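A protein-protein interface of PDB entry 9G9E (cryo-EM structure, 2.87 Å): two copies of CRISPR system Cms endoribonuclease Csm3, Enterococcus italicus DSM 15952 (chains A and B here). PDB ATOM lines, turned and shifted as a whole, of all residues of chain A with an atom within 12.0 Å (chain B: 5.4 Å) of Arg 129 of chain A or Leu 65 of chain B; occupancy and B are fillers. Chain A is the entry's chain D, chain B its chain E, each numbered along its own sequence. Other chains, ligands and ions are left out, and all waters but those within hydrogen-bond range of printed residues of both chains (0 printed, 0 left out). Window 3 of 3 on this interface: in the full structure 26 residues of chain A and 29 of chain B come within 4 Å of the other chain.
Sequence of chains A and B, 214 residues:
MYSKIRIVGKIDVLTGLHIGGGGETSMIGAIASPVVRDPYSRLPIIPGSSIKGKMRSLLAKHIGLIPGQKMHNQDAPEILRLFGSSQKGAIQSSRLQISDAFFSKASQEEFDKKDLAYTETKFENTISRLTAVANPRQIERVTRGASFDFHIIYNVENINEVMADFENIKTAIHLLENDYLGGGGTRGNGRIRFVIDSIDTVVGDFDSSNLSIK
ND1 of His 72 of chain B sits at hydrogen-bond distance from NH2 of Arg 129 of chain A (3.4 Å). A ring nitrogen (NE2) of His 72 of chain B is in hydrogen-bond range of the backbone carbonyl oxygen (O) of Ile 127 of chain A, 3.1 Å away. OD2 of Asp 75 of chain B is in salt-bridge range of NH2 of Arg 129 of chain A, at 3.3 Å.
The guanidinium group (NE) of Arg 56 of chain B is in salt-bridge range of the side-chain carboxylate (OD2) of Asp 75 of chain B, at 3.3 Å. The side-chain amide nitrogen (NE2) of Gln 69 of chain B lies within hydrogen-bond range of the backbone carbonyl oxygen (O) of Met 71 of chain B (2.8 Å). NH2 of Arg 56 of chain B sits at hydrogen-bond distance from O of His 72 of chain B (2.9 Å). The side-chain hydroxyl of Ser 128 of chain A lies within hydrogen-bond range of the backbone NH of Leu 130 of chain A (2.9 Å). The side-chain amide nitrogen (NE2) of Gln 69 of chain B is in hydrogen-bond range of the side-chain carboxylate (OD1) of Asp 75 of chain B (2.8 Å).
Of the 14 printed residues of chain B, 7 touch a printed residue of chain A. Hydrophobic or aromatic side chains of chain B within 4 Å of the printed part of chain A: Leu 65 and His 72. Along chain B the printed residues that touch a printed residue of chain A span positions 56 to 75. Of the 12 printed residues of chain A, 3 touch a printed residue of chain B. Hydrophobic or aromatic side chains of chain A within 4 Å of the printed part of chain B: Leu 130. Among the printed residues, Asp or Glu carboxylates within 4 Å of a Lys or Arg side-chain nitrogen of the other chain: Arg 129 of chain A with Asp 75 of chain B (3.3 Å).
Among the printed residues, pairs that only touch across the chains: Arg 129 of chain A with Arg 56 of chain B, Arg 129 of chain A with Ser 57 of chain B, Arg 129 of chain A with Leu 65 of chain B, Arg 129 of chain A with Gln 69 of chain B, Leu 130 of chain A with Gln 69 of chain B and Leu 130 of chain A with Lys 70 of chain B.
Thr 126 of chain A touches none of the printed residues of chain B. Of the printed residues of chain B, Ile 127 of chain A touches His 72. Printed residues of chain B within 4 Å of Arg 129 of chain A: Arg 56 (3.7 Å), Ser 57 (3.9 Å), Leu 65 (3.99 Å), Gln 69 (3.6 Å), His 72 (3.4 Å) and Asp 75 (3.3 Å). Of the printed residues of chain B, Leu 130 of chain A touches Gln 69 and Lys 70. Arg 56 of chain B touches one residue of chain A. Of chain A, only Arg 129 (3.9 Å) comes within 4 Å of Ser 57 of chain B. No residue of chain A comes within 4 Å of Ala 60 of chain B. No residue of chain A comes within 4 Å of Gly 64 of chain B. Of the printed residues of chain A, Leu 65 of chain B touches Arg 129. No residue of chain A comes within 4 Å of Ile 66 of chain B. Of chain A, only Arg 129 (3.6 Å) and Leu 130 (3.2 Å) come within 4 Å of Gln 69 of chain B. Of the printed residues of chain A, Lys 70 of chain B touches Leu 130. His 72 of chain B touches just these residues of chain A: Ile 127 (3.1 Å) and Arg 129 (3.4 Å). Of the printed residues of chain A, Asp 75 of chain B touches Arg 129 (3.3 Å). The nearest printed residue of chain B that does not touch Arg 129 of chain A is Ala 60 of chain B (4.04 Å). The nearest printed residue of chain B that does not touch Leu 130 of chain A is Pro 67 of chain B (5.9 Å).
No position is printed for both chains. Of the 9 pairs that touch across the chains among the printed residues, none has its exchanged pair printed and touching as well.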
ATOM      1  N   ASN A 125     -20.999  -6.270  12.364  1.00  0.00           N
ATOM      2  CA  ASN A 125     -21.024  -5.671  13.685  1.00  0.00           C
ATOM      3  C   ASN A 125     -20.980  -6.757  14.750  1.00  0.00           C
ATOM      4  O   ASN A 125     -21.240  -7.933  14.485  1.00  0.00           O
ATOM      5  CB  ASN A 125     -22.275  -4.808  13.877  1.00  0.00           C
ATOM      6  CG  ASN A 125     -22.009  -3.338  13.651  1.00  0.00           C
ATOM      7  OD1 ASN A 125     -20.862  -2.919  13.498  1.00  0.00           O
ATOM      8  ND2 ASN A 125     -23.070  -2.541  13.631  1.00  0.00           N
ATOM      9  N   THR A 126     -20.613  -6.346  15.959  1.00  0.00           N
ATOM     10  CA  THR A 126     -20.771  -7.169  17.155  1.00  0.00           C
ATOM     11  C   THR A 126     -21.292  -6.262  18.258  1.00  0.00           C
ATOM     12  O   THR A 126     -20.545  -5.430  18.781  1.00  0.00           O
ATOM     13  CB  THR A 126     -19.457  -7.833  17.562  1.00  0.00           C
ATOM     14  OG1 THR A 126     -19.038  -8.733  16.531  1.00  0.00           O
ATOM     15  CG2 THR A 126     -19.634  -8.606  18.859  1.00  0.00           C
ATOM     16  N   ILE A 127     -22.570  -6.397  18.588  1.00  0.00           N
ATOM     17  CA  ILE A 127     -23.203  -5.565  19.603  1.00  0.00           C
ATOM     18  C   ILE A 127     -22.922  -6.190  20.962  1.00  0.00           C
ATOM     19  O   ILE A 127     -23.266  -7.352  21.205  1.00  0.00           O
ATOM     20  CB  ILE A 127     -24.713  -5.424  19.353  1.00  0.00           C
ATOM     21  CG1 ILE A 127     -24.985  -4.366  18.279  1.00  0.00           C
ATOM     22  CG2 ILE A 127     -25.439  -5.054  20.636  1.00  0.00           C
ATOM     23  CD1 ILE A 127     -24.820  -4.862  16.857  1.00  0.00           C
ATOM     24  N   SER A 128     -22.285  -5.423  21.842  1.00  0.00           N
ATOM     25  CA  SER A 128     -21.917  -5.931  23.153  1.00  0.00           C
ATOM     26  C   SER A 128     -23.156  -6.204  23.997  1.00  0.00           C
ATOM     27  O   SER A 128     -24.153  -5.481  23.935  1.00  0.00           O
ATOM     28  CB  SER A 128     -21.002  -4.937  23.870  1.00  0.00           C
ATOM     29  OG  SER A 128     -21.219  -4.961  25.269  1.00  0.00           O
ATOM     30  N   ARG A 129     -23.082  -7.269  24.796  1.00  0.00           N
ATOM     31  CA  ARG A 129     -24.175  -7.638  25.686  1.00  0.00           C
ATOM     32  C   ARG A 129     -24.268  -6.744  26.914  1.00  0.00           C
ATOM     33  O   ARG A 129     -25.248  -6.845  27.658  1.00  0.00           O
ATOM     34  CB  ARG A 129     -24.024  -9.095  26.125  1.00  0.00           C
ATOM     35  CG  ARG A 129     -24.458 -10.113  25.085  1.00  0.00           C
ATOM     36  CD  ARG A 129     -25.967 -10.289  25.082  1.00  0.00           C
ATOM     37  NE  ARG A 129     -26.389 -11.378  24.209  1.00  0.00           N
ATOM     38  CZ  ARG A 129     -26.778 -11.222  22.951  1.00  0.00           C
ATOM     39  NH1 ARG A 129     -26.817 -10.029  22.383  1.00  0.00           N
ATOM     40  NH2 ARG A 129     -27.138 -12.290  22.247  1.00  0.00           N
ATOM     41  N   LEU A 130     -23.279  -5.880  27.144  1.00  0.00           N
ATOM     42  CA  LEU A 130     -23.251  -5.014  28.314  1.00  0.00           C
ATOM     43  C   LEU A 130     -23.454  -3.548  27.953  1.00  0.00           C
ATOM     44  O   LEU A 130     -24.374  -2.906  28.466  1.00  0.00           O
ATOM     45  CB  LEU A 130     -21.924  -5.198  29.064  1.00  0.00           C
ATOM     46  CG  LEU A 130     -21.825  -4.551  30.446  1.00  0.00           C
ATOM     47  CD1 LEU A 130     -22.853  -5.148  31.393  1.00  0.00           C
ATOM     48  CD2 LEU A 130     -20.420  -4.699  31.008  1.00  0.00           C
ATOM     49  N   THR A 131     -22.616  -2.999  27.074  1.00  0.00           N
ATOM     50  CA  THR A 131     -22.676  -1.587  26.725  1.00  0.00           C
ATOM     51  C   THR A 131     -23.506  -1.305  25.481  1.00  0.00           C
ATOM     52  O   THR A 131     -23.712  -0.131  25.152  1.00  0.00           O
ATOM     53  CB  THR A 131     -21.261  -1.031  26.518  1.00  0.00           C
ATOM     54  OG1 THR A 131     -20.600  -1.773  25.485  1.00  0.00           O
ATOM     55  CG2 THR A 131     -20.455  -1.136  27.804  1.00  0.00           C
ATOM     56  N   ALA A 132     -23.987  -2.342  24.792  1.00  0.00           N
ATOM     57  CA  ALA A 132     -24.753  -2.185  23.553  1.00  0.00           C
ATOM     58  C   ALA A 132     -23.986  -1.350  22.531  1.00  0.00           C
ATOM     59  O   ALA A 132     -24.551  -0.507  21.832  1.00  0.00           O
ATOM     60  CB  ALA A 132     -26.133  -1.585  23.829  1.00  0.00           C
ATOM     61  N   VAL A 133     -22.680  -1.591  22.445  1.00  0.00           N
ATOM     62  CA  VAL A 133     -21.790  -0.871  21.542  1.00  0.00           C
ATOM     63  C   VAL A 133     -21.347  -1.831  20.449  1.00  0.00           C
ATOM     64  O   VAL A 133     -20.881  -2.940  20.739  1.00  0.00           O
ATOM     65  CB  VAL A 133     -20.579  -0.286  22.289  1.00  0.00           C
ATOM     66  CG1 VAL A 133     -19.559   0.262  21.304  1.00  0.00           C
ATOM     67  CG2 VAL A 133     -21.026   0.799  23.256  1.00  0.00           C
ATOM     68  N   ALA A 134     -21.491  -1.407  19.197  1.00  0.00           N
ATOM     69  CA  ALA A 134     -21.201  -2.259  18.053  1.00  0.00           C
ATOM     70  C   ALA A 134     -19.734  -2.126  17.663  1.00  0.00           C
ATOM     71  O   ALA A 134     -19.289  -1.049  17.249  1.00  0.00           O
ATOM     72  CB  ALA A 134     -22.104  -1.904  16.873  1.00  0.00           C
ATOM     73  N   ASN A 135     -18.990  -3.222  17.797  1.00  0.00           N
ATOM     74  CA  ASN A 135     -17.616  -3.299  17.330  1.00  0.00           C
ATOM     75  C   ASN A 135     -17.617  -3.738  15.878  1.00  0.00           C
ATOM     76  O   ASN A 135     -18.177  -4.802  15.568  1.00  0.00           O
ATOM     77  CB  ASN A 135     -16.817  -4.281  18.180  1.00  0.00           C
ATOM     78  CG  ASN A 135     -15.343  -4.295  17.830  1.00  0.00           C
ATOM     79  OD1 ASN A 135     -14.807  -3.319  17.306  1.00  0.00           O
ATOM     80  ND2 ASN A 135     -14.679  -5.408  18.116  1.00  0.00           N
ATOM     81  N   ARG A 187     -23.422 -17.957   9.997  1.00  0.00           N
ATOM     82  CA  ARG A 187     -23.834 -16.587   9.720  1.00  0.00           C
ATOM     83  C   ARG A 187     -23.855 -16.316   8.217  1.00  0.00           C
ATOM     84  O   ARG A 187     -23.499 -15.229   7.758  1.00  0.00           O
ATOM     85  CB  ARG A 187     -22.922 -15.597  10.439  1.00  0.00           C
ATOM     86  CG  ARG A 187     -22.895 -15.777  11.949  1.00  0.00           C
ATOM     87  CD  ARG A 187     -21.893 -14.843  12.613  1.00  0.00           C
ATOM     88  NE  ARG A 187     -20.520 -15.116  12.205  1.00  0.00           N
ATOM     89  CZ  ARG A 187     -19.799 -16.150  12.620  1.00  0.00           C
ATOM     90  NH1 ARG A 187     -20.289 -17.042  13.463  1.00  0.00           N
ATOM     91  NH2 ARG A 187     -18.552 -16.290  12.178  1.00  0.00           N
ATOM     92  N   ARG B  56     -30.848 -14.034  17.807  1.00  0.00           N
ATOM     93  CA  ARG B  56     -30.180 -14.406  19.048  1.00  0.00           C
ATOM     94  C   ARG B  56     -30.378 -13.347  20.123  1.00  0.00           C
ATOM     95  O   ARG B  56     -30.638 -13.678  21.283  1.00  0.00           O
ATOM     96  CB  ARG B  56     -28.692 -14.639  18.790  1.00  0.00           C
ATOM     97  CG  ARG B  56     -27.931 -15.177  19.987  1.00  0.00           C
ATOM     98  CD  ARG B  56     -26.436 -14.963  19.830  1.00  0.00           C
ATOM     99  NE  ARG B  56     -25.682 -15.547  20.933  1.00  0.00           N
ATOM    100  CZ  ARG B  56     -24.889 -16.603  20.820  1.00  0.00           C
ATOM    101  NH1 ARG B  56     -24.717 -17.217  19.662  1.00  0.00           N
ATOM    102  NH2 ARG B  56     -24.252 -17.055  21.896  1.00  0.00           N
ATOM    103  N   SER B  57     -30.265 -12.069  19.756  1.00  0.00           N
ATOM    104  CA  SER B  57     -30.448 -10.998  20.730  1.00  0.00           C
ATOM    105  C   SER B  57     -31.872 -10.983  21.271  1.00  0.00           C
ATOM    106  O   SER B  57     -32.087 -10.869  22.484  1.00  0.00           O
ATOM    107  CB  SER B  57     -30.097  -9.651  20.097  1.00  0.00           C
ATOM    108  OG  SER B  57     -30.468  -8.577  20.943  1.00  0.00           O
ATOM    109  N   ALA B  60     -32.393 -14.045  23.525  1.00  0.00           N
ATOM    110  CA  ALA B  60     -31.695 -13.877  24.794  1.00  0.00           C
ATOM    111  C   ALA B  60     -32.426 -12.895  25.699  1.00  0.00           C
ATOM    112  O   ALA B  60     -32.534 -13.119  26.910  1.00  0.00           O
ATOM    113  CB  ALA B  60     -30.260 -13.415  24.547  1.00  0.00           C
ATOM    114  N   LYS B  61     -32.928 -11.795  25.131  1.00  0.00           N
ATOM    115  CA  LYS B  61     -33.682 -10.836  25.934  1.00  0.00           C
ATOM    116  C   LYS B  61     -34.977 -11.445  26.456  1.00  0.00           C
ATOM    117  O   LYS B  61     -35.349 -11.228  27.615  1.00  0.00           O
ATOM    118  CB  LYS B  61     -33.973  -9.578  25.115  1.00  0.00           C
ATOM    119  CG  LYS B  61     -32.785  -8.640  24.977  1.00  0.00           C
ATOM    120  CD  LYS B  61     -33.203  -7.304  24.383  1.00  0.00           C
ATOM    121  CE  LYS B  61     -33.968  -7.490  23.083  1.00  0.00           C
ATOM    122  NZ  LYS B  61     -34.382  -6.189  22.490  1.00  0.00           N
ATOM    123  N   ILE B  63     -35.825 -14.802  26.843  1.00  0.00           N
ATOM    124  CA  ILE B  63     -35.587 -15.893  27.783  1.00  0.00           C
ATOM    125  C   ILE B  63     -35.019 -15.358  29.092  1.00  0.00           C
ATOM    126  O   ILE B  63     -35.438 -15.770  30.181  1.00  0.00           O
ATOM    127  CB  ILE B  63     -34.667 -16.949  27.143  1.00  0.00           C
ATOM    128  CG1 ILE B  63     -35.475 -17.853  26.210  1.00  0.00           C
ATOM    129  CG2 ILE B  63     -33.957 -17.768  28.211  1.00  0.00           C
ATOM    130  CD1 ILE B  63     -34.724 -19.073  25.731  1.00  0.00           C
ATOM    131  N   GLY B  64     -34.071 -14.429  29.010  1.00  0.00           N
ATOM    132  CA  GLY B  64     -33.476 -13.848  30.196  1.00  0.00           C
ATOM    133  C   GLY B  64     -32.005 -13.530  30.029  1.00  0.00           C
ATOM    134  O   GLY B  64     -31.231 -14.364  29.551  1.00  0.00           O
ATOM    135  N   LEU B  65     -31.611 -12.322  30.420  1.00  0.00           N
ATOM    136  CA  LEU B  65     -30.232 -11.866  30.314  1.00  0.00           C
ATOM    137  C   LEU B  65     -29.596 -11.848  31.696  1.00  0.00           C
ATOM    138  O   LEU B  65     -30.139 -11.243  32.626  1.00  0.00           O
ATOM    139  CB  LEU B  65     -30.165 -10.474  29.680  1.00  0.00           C
ATOM    140  CG  LEU B  65     -28.963 -10.192  28.776  1.00  0.00           C
ATOM    141  CD1 LEU B  65     -29.140 -10.865  27.425  1.00  0.00           C
ATOM    142  CD2 LEU B  65     -28.755  -8.696  28.610  1.00  0.00           C
ATOM    143  N   ILE B  66     -28.454 -12.515  31.825  1.00  0.00           N
ATOM    144  CA  ILE B  66     -27.740 -12.534  33.107  1.00  0.00           C
ATOM    145  C   ILE B  66     -27.247 -11.128  33.427  1.00  0.00           C
ATOM    146  O   ILE B  66     -26.683 -10.454  32.542  1.00  0.00           O
ATOM    147  CB  ILE B  66     -26.568 -13.529  33.056  1.00  0.00           C
ATOM    148  CG1 ILE B  66     -27.022 -14.864  32.461  1.00  0.00           C
ATOM    149  CG2 ILE B  66     -25.978 -13.733  34.443  1.00  0.00           C
ATOM    150  CD1 ILE B  66     -28.140 -15.532  33.233  1.00  0.00           C
ATOM    151  N   PRO B  67     -27.445 -10.625  34.645  1.00  0.00           N
ATOM    152  CA  PRO B  67     -26.931  -9.293  34.983  1.00  0.00           C
ATOM    153  C   PRO B  67     -25.413  -9.237  34.866  1.00  0.00           C
ATOM    154  O   PRO B  67     -24.708 -10.185  35.214  1.00  0.00           O
ATOM    155  CB  PRO B  67     -27.392  -9.089  36.431  1.00  0.00           C
ATOM    156  CG  PRO B  67     -28.556 -10.013  36.593  1.00  0.00           C
ATOM    157  CD  PRO B  67     -28.245 -11.205  35.738  1.00  0.00           C
ATOM    158  N   GLN B  69     -23.685  -9.328  32.207  1.00  0.00           N
ATOM    159  CA  GLN B  69     -23.168 -10.177  31.144  1.00  0.00           C
ATOM    160  C   GLN B  69     -22.337  -9.362  30.162  1.00  0.00           C
ATOM    161  O   GLN B  69     -22.703  -8.244  29.791  1.00  0.00           O
ATOM    162  CB  GLN B  69     -24.318 -10.869  30.416  1.00  0.00           C
ATOM    163  CG  GLN B  69     -23.878 -11.820  29.324  1.00  0.00           C
ATOM    164  CD  GLN B  69     -25.040 -12.564  28.703  1.00  0.00           C
ATOM    165  OE1 GLN B  69     -26.176 -12.466  29.166  1.00  0.00           O
ATOM    166  NE2 GLN B  69     -24.760 -13.319  27.651  1.00  0.00           N
ATOM    167  N   LYS B  70     -21.211  -9.933  29.737  1.00  0.00           N
ATOM    168  CA  LYS B  70     -20.294  -9.261  28.827  1.00  0.00           C
ATOM    169  C   LYS B  70     -20.083  -9.988  27.510  1.00  0.00           C
ATOM    170  O   LYS B  70     -19.826  -9.334  26.498  1.00  0.00           O
ATOM    171  CB  LYS B  70     -18.927  -9.058  29.499  1.00  0.00           C
ATOM    172  CG  LYS B  70     -18.943  -8.079  30.658  1.00  0.00           C
ATOM    173  CD  LYS B  70     -17.562  -7.934  31.273  1.00  0.00           C
ATOM    174  CE  LYS B  70     -17.076  -9.254  31.846  1.00  0.00           C
ATOM    175  NZ  LYS B  70     -18.031  -9.806  32.846  1.00  0.00           N
ATOM    176  N   MET B  71     -20.184 -11.314  27.489  1.00  0.00           N
ATOM    177  CA  MET B  71     -19.941 -12.101  26.292  1.00  0.00           C
ATOM    178  C   MET B  71     -21.207 -12.843  25.889  1.00  0.00           C
ATOM    179  O   MET B  71     -22.077 -13.129  26.716  1.00  0.00           O
ATOM    180  CB  MET B  71     -18.801 -13.104  26.508  1.00  0.00           C
ATOM    181  CG  MET B  71     -17.432 -12.469  26.688  1.00  0.00           C
ATOM    182  SD  MET B  71     -16.086 -13.670  26.647  1.00  0.00           S
ATOM    183  CE  MET B  71     -16.969 -15.199  26.957  1.00  0.00           C
ATOM    184  N   HIS B  72     -21.300 -13.158  24.596  1.00  0.00           N
ATOM    185  CA  HIS B  72     -22.423 -13.938  24.093  1.00  0.00           C
ATOM    186  C   HIS B  72     -22.390 -15.381  24.573  1.00  0.00           C
ATOM    187  O   HIS B  72     -23.426 -16.056  24.539  1.00  0.00           O
ATOM    188  CB  HIS B  72     -22.450 -13.905  22.564  1.00  0.00           C
ATOM    189  CG  HIS B  72     -22.720 -12.547  21.993  1.00  0.00           C
ATOM    190  ND1 HIS B  72     -23.861 -12.255  21.280  1.00  0.00           N
ATOM    191  CD2 HIS B  72     -21.998 -11.403  22.034  1.00  0.00           C
ATOM    192  CE1 HIS B  72     -23.832 -10.989  20.905  1.00  0.00           C
ATOM    193  NE2 HIS B  72     -22.712 -10.449  21.350  1.00  0.00           N
ATOM    194  N   ASP B  75     -24.878 -16.517  27.526  1.00  0.00           N
ATOM    195  CA  ASP B  75     -26.316 -16.587  27.318  1.00  0.00           C
ATOM    196  C   ASP B  75     -26.892 -17.835  27.988  1.00  0.00           C
ATOM    197  O   ASP B  75     -26.182 -18.639  28.598  1.00  0.00           O
ATOM    198  CB  ASP B  75     -26.634 -16.581  25.825  1.00  0.00           C
ATOM    199  CG  ASP B  75     -26.751 -15.182  25.254  1.00  0.00           C
ATOM    200  OD1 ASP B  75     -26.847 -14.221  26.042  1.00  0.00           O
ATOM    201  OD2 ASP B  75     -26.740 -15.043  24.013  1.00  0.00           O
